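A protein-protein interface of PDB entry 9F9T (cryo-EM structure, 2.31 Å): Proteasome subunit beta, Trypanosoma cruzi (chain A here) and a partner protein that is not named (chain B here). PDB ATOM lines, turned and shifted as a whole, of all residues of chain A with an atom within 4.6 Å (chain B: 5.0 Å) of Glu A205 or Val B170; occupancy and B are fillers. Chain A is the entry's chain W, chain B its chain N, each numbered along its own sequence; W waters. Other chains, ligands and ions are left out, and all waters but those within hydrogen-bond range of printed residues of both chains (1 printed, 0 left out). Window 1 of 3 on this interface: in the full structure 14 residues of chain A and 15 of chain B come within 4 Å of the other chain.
CD2 of Leu B144 touches O of Ser A202, 3.7 Å away.
Val B170 touches Ser A202.
Val B170 touches Glu A205 (CG2 to CB, 3.8 Å).
OE1 of Glu A205 touches CD2 of Tyr B173, 3.1 Å away.
Thr A206 touches Leu B144.
Thr A206 touches Asp B166 (CG2 to CB, 3.9 Å).
CG2 of Val B170 touches CG2 of Thr A206, at 3.7 Å.
Water W1 lies within hydrogen-bond range of the backbone carbonyl oxygen of Phe A190 and the guanidinium group of Arg B174.
O of Val B140 lies close to OG of Ser A202 (3.4 Å).
The guanidinium group of Arg B174 lies within hydrogen-bond range of the side-chain sulfur of Met A201.
The guanidinium group (NH2) of Arg B174 lies within salt-bridge range of the side-chain carboxylate (OE2) of Glu A205 (2.7 Å).
The side-chain carboxylate (OD1) of Asp B166 is in salt-bridge range of the guanidinium group (NH2) of Arg B169 (2.7 Å).
O of Ser A202 is in hydrogen-bond range of OG1 of Thr A206, at 3.0 Å.
The side-chain hydroxyl (OG1) of Thr A206 lies within hydrogen-bond range of the backbone carbonyl oxygen (O) of Ala A203 (3.0 Å).
Ala A203 touches none of the printed residues of chain B.
Glu A205 touches just these residues of chain B: Val B170 (3.8 Å), Tyr B173 (3.1 Å) and Arg B174 (2.7 Å).
Printed residues of chain B within 4 Å of Thr A206: Leu B144, Asp B166 and Val B170.
Printed residues of chain A within 4 Å of Val B140: Ser A202 (3.4 Å).
Of chain A, only Ser A202, Glu A205 and Thr A206 come within 4 Å of Val B170.
Leu B171 touches none of the printed residues of chain A.
Printed residues of chain A within 4 Å of Tyr B173: Glu A205.
Of the printed residues of chain A, Arg B174 touches Met A201 and Glu A205.
The nearest printed residue of chain B that does not touch Glu A205 is Arg B169 (5.2 Å).
The nearest printed residue of chain A that does not touch Tyr B173 is Thr A206 (6.2 Å).
Printed residues of chain B that touch a printed residue of chain A: Val B140, Leu B144, Asp B166, Val B170, Tyr B173 and Arg B174.
Hydrophobic or aromatic side chains of chain A within 4 Å of the printed part of chain B: Met A201.
Among the printed residues, 10 pairs touch across the chains.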
ATOM      1  N   PHE A 190       0.757  30.838 -23.255  1.00  0.00           N
ATOM      2  CA  PHE A 190       0.636  29.585 -22.538  1.00  0.00           C
ATOM      3  C   PHE A 190       1.630  28.597 -23.116  1.00  0.00           C
ATOM      4  O   PHE A 190       1.830  28.625 -24.293  1.00  0.00           O
ATOM      5  CB  PHE A 190      -0.786  29.032 -22.580  1.00  0.00           C
ATOM      6  CG  PHE A 190      -1.412  28.880 -23.941  1.00  0.00           C
ATOM      7  CD1 PHE A 190      -2.039  29.934 -24.564  1.00  0.00           C
ATOM      8  CD2 PHE A 190      -1.422  27.667 -24.590  1.00  0.00           C
ATOM      9  CE1 PHE A 190      -2.623  29.796 -25.816  1.00  0.00           C
ATOM     10  CE2 PHE A 190      -2.110  27.486 -25.775  1.00  0.00           C
ATOM     11  CZ  PHE A 190      -2.676  28.567 -26.426  1.00  0.00           C
ATOM     12  N   MET A 201      -1.079  20.205 -22.993  1.00  0.00           N
ATOM     13  CA  MET A 201      -1.301  21.235 -24.018  1.00  0.00           C
ATOM     14  C   MET A 201      -2.695  21.150 -24.622  1.00  0.00           C
ATOM     15  O   MET A 201      -3.201  22.150 -25.144  1.00  0.00           O
ATOM     16  CB  MET A 201      -0.245  21.184 -25.127  1.00  0.00           C
ATOM     17  CG  MET A 201      -0.513  22.144 -26.338  1.00  0.00           C
ATOM     18  SD  MET A 201      -0.602  23.937 -25.808  1.00  0.00           S
ATOM     19  CE  MET A 201       1.105  24.223 -25.339  1.00  0.00           C
ATOM     20  N   SER A 202      -3.313  19.983 -24.454  1.00  0.00           N
ATOM     21  CA  SER A 202      -4.670  19.824 -24.932  1.00  0.00           C
ATOM     22  C   SER A 202      -5.676  20.403 -23.959  1.00  0.00           C
ATOM     23  O   SER A 202      -6.777  20.719 -24.314  1.00  0.00           O
ATOM     24  CB  SER A 202      -4.926  18.376 -25.168  1.00  0.00           C
ATOM     25  OG  SER A 202      -5.378  17.755 -23.972  1.00  0.00           O
ATOM     26  N   ALA A 203      -5.347  20.488 -22.689  1.00  0.00           N
ATOM     27  CA  ALA A 203      -6.194  21.205 -21.756  1.00  0.00           C
ATOM     28  C   ALA A 203      -6.056  22.699 -21.979  1.00  0.00           C
ATOM     29  O   ALA A 203      -7.014  23.432 -21.927  1.00  0.00           O
ATOM     30  CB  ALA A 203      -5.796  20.817 -20.362  1.00  0.00           C
ATOM     31  N   LEU A 204      -4.821  23.170 -22.145  1.00  0.00           N
ATOM     32  CA  LEU A 204      -4.592  24.577 -22.404  1.00  0.00           C
ATOM     33  C   LEU A 204      -5.278  25.101 -23.680  1.00  0.00           C
ATOM     34  O   LEU A 204      -5.819  26.189 -23.645  1.00  0.00           O
ATOM     35  CB  LEU A 204      -3.098  24.819 -22.504  1.00  0.00           C
ATOM     36  CG  LEU A 204      -2.296  24.506 -21.246  1.00  0.00           C
ATOM     37  CD1 LEU A 204      -0.813  24.760 -21.500  1.00  0.00           C
ATOM     38  CD2 LEU A 204      -2.764  25.374 -20.092  1.00  0.00           C
ATOM     39  N   GLU A 205      -5.241  24.432 -24.808  1.00  0.00           N
ATOM     40  CA  GLU A 205      -5.912  24.972 -25.973  1.00  0.00           C
ATOM     41  C   GLU A 205      -7.428  24.923 -25.860  1.00  0.00           C
ATOM     42  O   GLU A 205      -8.130  25.605 -26.593  1.00  0.00           O
ATOM     43  CB  GLU A 205      -5.632  24.159 -27.227  1.00  0.00           C
ATOM     44  CG  GLU A 205      -4.189  24.223 -27.731  1.00  0.00           C
ATOM     45  CD  GLU A 205      -3.764  25.428 -28.543  1.00  0.00           C
ATOM     46  OE1 GLU A 205      -4.649  26.291 -28.791  1.00  0.00           O
ATOM     47  OE2 GLU A 205      -2.580  25.496 -28.965  1.00  0.00           O
ATOM     48  N   THR A 206      -7.998  24.059 -25.032  1.00  0.00           N
ATOM     49  CA  THR A 206      -9.445  24.101 -24.939  1.00  0.00           C
ATOM     50  C   THR A 206      -9.894  25.108 -23.910  1.00  0.00           C
ATOM     51  O   THR A 206     -11.073  25.413 -23.908  1.00  0.00           O
ATOM     52  CB  THR A 206      -9.987  22.736 -24.610  1.00  0.00           C
ATOM     53  OG1 THR A 206      -9.274  22.189 -23.504  1.00  0.00           O
ATOM     54  CG2 THR A 206      -9.622  21.793 -25.719  1.00  0.00           C
ATOM     55  N   GLY A 207      -8.999  25.541 -23.019  1.00  0.00           N
ATOM     56  CA  GLY A 207      -9.423  26.281 -21.852  1.00  0.00           C
ATOM     57  C   GLY A 207      -8.807  27.668 -21.686  1.00  0.00           C
ATOM     58  O   GLY A 207      -9.223  28.399 -20.808  1.00  0.00           O
ATOM     59  N   VAL B 140      -3.269  13.428 -27.626  1.00  0.00           N
ATOM     60  CA  VAL B 140      -3.908  14.735 -27.612  1.00  0.00           C
ATOM     61  C   VAL B 140      -5.387  14.615 -27.204  1.00  0.00           C
ATOM     62  O   VAL B 140      -5.899  15.405 -26.422  1.00  0.00           O
ATOM     63  CB  VAL B 140      -3.812  15.386 -29.002  1.00  0.00           C
ATOM     64  CG1 VAL B 140      -4.804  16.515 -29.189  1.00  0.00           C
ATOM     65  CG2 VAL B 140      -2.443  15.931 -29.364  1.00  0.00           C
ATOM     66  N   LEU B 144      -8.588  14.404 -22.957  1.00  0.00           N
ATOM     67  CA  LEU B 144      -9.852  15.093 -22.883  1.00  0.00           C
ATOM     68  C   LEU B 144     -11.073  14.201 -22.807  1.00  0.00           C
ATOM     69  O   LEU B 144     -12.049  14.637 -22.210  1.00  0.00           O
ATOM     70  CB  LEU B 144     -10.060  15.951 -24.119  1.00  0.00           C
ATOM     71  CG  LEU B 144      -9.110  17.106 -24.333  1.00  0.00           C
ATOM     72  CD1 LEU B 144      -9.539  17.890 -25.567  1.00  0.00           C
ATOM     73  CD2 LEU B 144      -9.079  18.030 -23.113  1.00  0.00           C
ATOM     74  N   ASP B 166     -13.763  19.582 -29.532  1.00  0.00           N
ATOM     75  CA  ASP B 166     -12.627  20.181 -28.855  1.00  0.00           C
ATOM     76  C   ASP B 166     -11.340  19.410 -29.148  1.00  0.00           C
ATOM     77  O   ASP B 166     -10.279  20.013 -29.310  1.00  0.00           O
ATOM     78  CB  ASP B 166     -12.877  20.284 -27.348  1.00  0.00           C
ATOM     79  CG  ASP B 166     -13.943  21.321 -26.940  1.00  0.00           C
ATOM     80  OD1 ASP B 166     -14.539  22.003 -27.849  1.00  0.00           O
ATOM     81  OD2 ASP B 166     -14.180  21.472 -25.700  1.00  0.00           O
ATOM     82  N   CYS B 167     -11.436  18.063 -29.200  1.00  0.00           N
ATOM     83  CA  CYS B 167     -10.272  17.250 -29.546  1.00  0.00           C
ATOM     84  C   CYS B 167      -9.849  17.531 -30.999  1.00  0.00           C
ATOM     85  O   CYS B 167      -8.676  17.736 -31.303  1.00  0.00           O
ATOM     86  CB  CYS B 167     -10.575  15.760 -29.421  1.00  0.00           C
ATOM     87  SG  CYS B 167     -11.062  15.164 -27.777  1.00  0.00           S
ATOM     88  N   LEU B 168     -10.840  17.551 -31.911  1.00  0.00           N
ATOM     89  CA  LEU B 168     -10.555  17.863 -33.307  1.00  0.00           C
ATOM     90  C   LEU B 168      -9.800  19.191 -33.411  1.00  0.00           C
ATOM     91  O   LEU B 168      -8.788  19.251 -34.107  1.00  0.00           O
ATOM     92  CB  LEU B 168     -11.813  17.862 -34.149  1.00  0.00           C
ATOM     93  CG  LEU B 168     -12.518  16.536 -34.211  1.00  0.00           C
ATOM     94  CD1 LEU B 168     -13.776  16.622 -35.039  1.00  0.00           C
ATOM     95  CD2 LEU B 168     -11.650  15.418 -34.739  1.00  0.00           C
ATOM     96  N   ARG B 169     -10.201  20.171 -32.599  1.00  0.00           N
ATOM     97  CA  ARG B 169      -9.630  21.490 -32.686  1.00  0.00           C
ATOM     98  C   ARG B 169      -8.168  21.507 -32.226  1.00  0.00           C
ATOM     99  O   ARG B 169      -7.294  22.050 -32.866  1.00  0.00           O
ATOM    100  CB  ARG B 169     -10.575  22.423 -31.962  1.00  0.00           C
ATOM    101  CG  ARG B 169     -10.063  23.842 -31.870  1.00  0.00           C
ATOM    102  CD  ARG B 169     -10.924  24.597 -30.858  1.00  0.00           C
ATOM    103  NE  ARG B 169     -12.277  24.696 -31.377  1.00  0.00           N
ATOM    104  CZ  ARG B 169     -13.355  24.149 -30.846  1.00  0.00           C
ATOM    105  NH1 ARG B 169     -14.533  24.315 -31.429  1.00  0.00           N
ATOM    106  NH2 ARG B 169     -13.290  23.414 -29.751  1.00  0.00           N
ATOM    107  N   VAL B 170      -7.886  20.765 -31.174  1.00  0.00           N
ATOM    108  CA  VAL B 170      -6.534  20.603 -30.747  1.00  0.00           C
ATOM    109  C   VAL B 170      -5.720  19.821 -31.761  1.00  0.00           C
ATOM    110  O   VAL B 170      -4.554  20.160 -31.915  1.00  0.00           O
ATOM    111  CB  VAL B 170      -6.462  19.951 -29.362  1.00  0.00           C
ATOM    112  CG1 VAL B 170      -5.019  19.747 -28.865  1.00  0.00           C
ATOM    113  CG2 VAL B 170      -7.196  20.839 -28.382  1.00  0.00           C
ATOM    114  N   LEU B 171      -6.231  18.779 -32.404  1.00  0.00           N
ATOM    115  CA  LEU B 171      -5.445  18.097 -33.421  1.00  0.00           C
ATOM    116  C   LEU B 171      -5.084  19.061 -34.548  1.00  0.00           C
ATOM    117  O   LEU B 171      -3.954  19.139 -34.981  1.00  0.00           O
ATOM    118  CB  LEU B 171      -6.246  16.930 -33.976  1.00  0.00           C
ATOM    119  CG  LEU B 171      -6.338  15.738 -33.020  1.00  0.00           C
ATOM    120  CD1 LEU B 171      -7.382  14.789 -33.480  1.00  0.00           C
ATOM    121  CD2 LEU B 171      -4.965  14.935 -32.872  1.00  0.00           C
ATOM    122  N   PHE B 172      -6.095  19.778 -35.019  1.00  0.00           N
ATOM    123  CA  PHE B 172      -5.881  20.760 -36.031  1.00  0.00           C
ATOM    124  C   PHE B 172      -4.842  21.760 -35.560  1.00  0.00           C
ATOM    125  O   PHE B 172      -3.999  22.122 -36.360  1.00  0.00           O
ATOM    126  CB  PHE B 172      -7.189  21.452 -36.404  1.00  0.00           C
ATOM    127  CG  PHE B 172      -6.946  22.471 -37.462  1.00  0.00           C
ATOM    128  CD1 PHE B 172      -6.346  22.099 -38.664  1.00  0.00           C
ATOM    129  CD2 PHE B 172      -7.139  23.816 -37.219  1.00  0.00           C
ATOM    130  CE1 PHE B 172      -6.028  23.051 -39.635  1.00  0.00           C
ATOM    131  CE2 PHE B 172      -6.872  24.761 -38.215  1.00  0.00           C
ATOM    132  CZ  PHE B 172      -6.318  24.382 -39.415  1.00  0.00           C
ATOM    133  N   TYR B 173      -4.816  22.165 -34.296  1.00  0.00           N
ATOM    134  CA  TYR B 173      -3.805  23.119 -33.892  1.00  0.00           C
ATOM    135  C   TYR B 173      -2.419  22.508 -33.740  1.00  0.00           C
ATOM    136  O   TYR B 173      -1.463  23.234 -33.951  1.00  0.00           O
ATOM    137  CB  TYR B 173      -3.968  23.827 -32.551  1.00  0.00           C
ATOM    138  CG  TYR B 173      -5.167  24.743 -32.374  1.00  0.00           C
ATOM    139  CD1 TYR B 173      -5.547  25.646 -33.349  1.00  0.00           C
ATOM    140  CD2 TYR B 173      -5.890  24.733 -31.200  1.00  0.00           C
ATOM    141  CE1 TYR B 173      -6.615  26.521 -33.160  1.00  0.00           C
ATOM    142  CE2 TYR B 173      -6.992  25.537 -31.009  1.00  0.00           C
ATOM    143  CZ  TYR B 173      -7.340  26.454 -31.976  1.00  0.00           C
ATOM    144  OH  TYR B 173      -8.430  27.257 -31.760  1.00  0.00           O
ATOM    145  N   ARG B 174      -2.270  21.249 -33.331  1.00  0.00           N
ATOM    146  CA  ARG B 174      -0.977  20.775 -32.872  1.00  0.00           C
ATOM    147  C   ARG B 174      -0.427  19.598 -33.656  1.00  0.00           C
ATOM    148  O   ARG B 174       0.741  19.271 -33.521  1.00  0.00           O
ATOM    149  CB  ARG B 174      -1.076  20.458 -31.389  1.00  0.00           C
ATOM    150  CG  ARG B 174      -1.492  21.630 -30.540  1.00  0.00           C
ATOM    151  CD  ARG B 174      -0.263  22.431 -30.250  1.00  0.00           C
ATOM    152  NE  ARG B 174      -0.568  23.740 -29.730  1.00  0.00           N
ATOM    153  CZ  ARG B 174       0.391  24.574 -29.366  1.00  0.00           C
ATOM    154  NH1 ARG B 174       1.666  24.251 -29.586  1.00  0.00           N
ATOM    155  NH2 ARG B 174       0.111  25.756 -28.859  1.00  0.00           N
ATOM    156  N   GLU B 175      -1.237  19.047 -34.538  1.00  0.00           N
ATOM    157  CA  GLU B 175      -0.787  17.968 -35.377  1.00  0.00           C
ATOM    158  C   GLU B 175      -0.407  18.562 -36.731  1.00  0.00           C
ATOM    159  O   GLU B 175      -1.227  19.136 -37.418  1.00  0.00           O
ATOM    160  CB  GLU B 175      -1.860  16.867 -35.382  1.00  0.00           C
ATOM    161  CG  GLU B 175      -1.529  15.671 -36.259  1.00  0.00           C
ATOM    162  CD  GLU B 175      -2.651  14.647 -36.467  1.00  0.00           C
ATOM    163  OE1 GLU B 175      -3.847  15.059 -36.420  1.00  0.00           O
ATOM    164  OE2 GLU B 175      -2.355  13.424 -36.709  1.00  0.00           O
HETATM  165  O   HOH W   1       2.723  26.935 -26.858  1.00  0.00           O
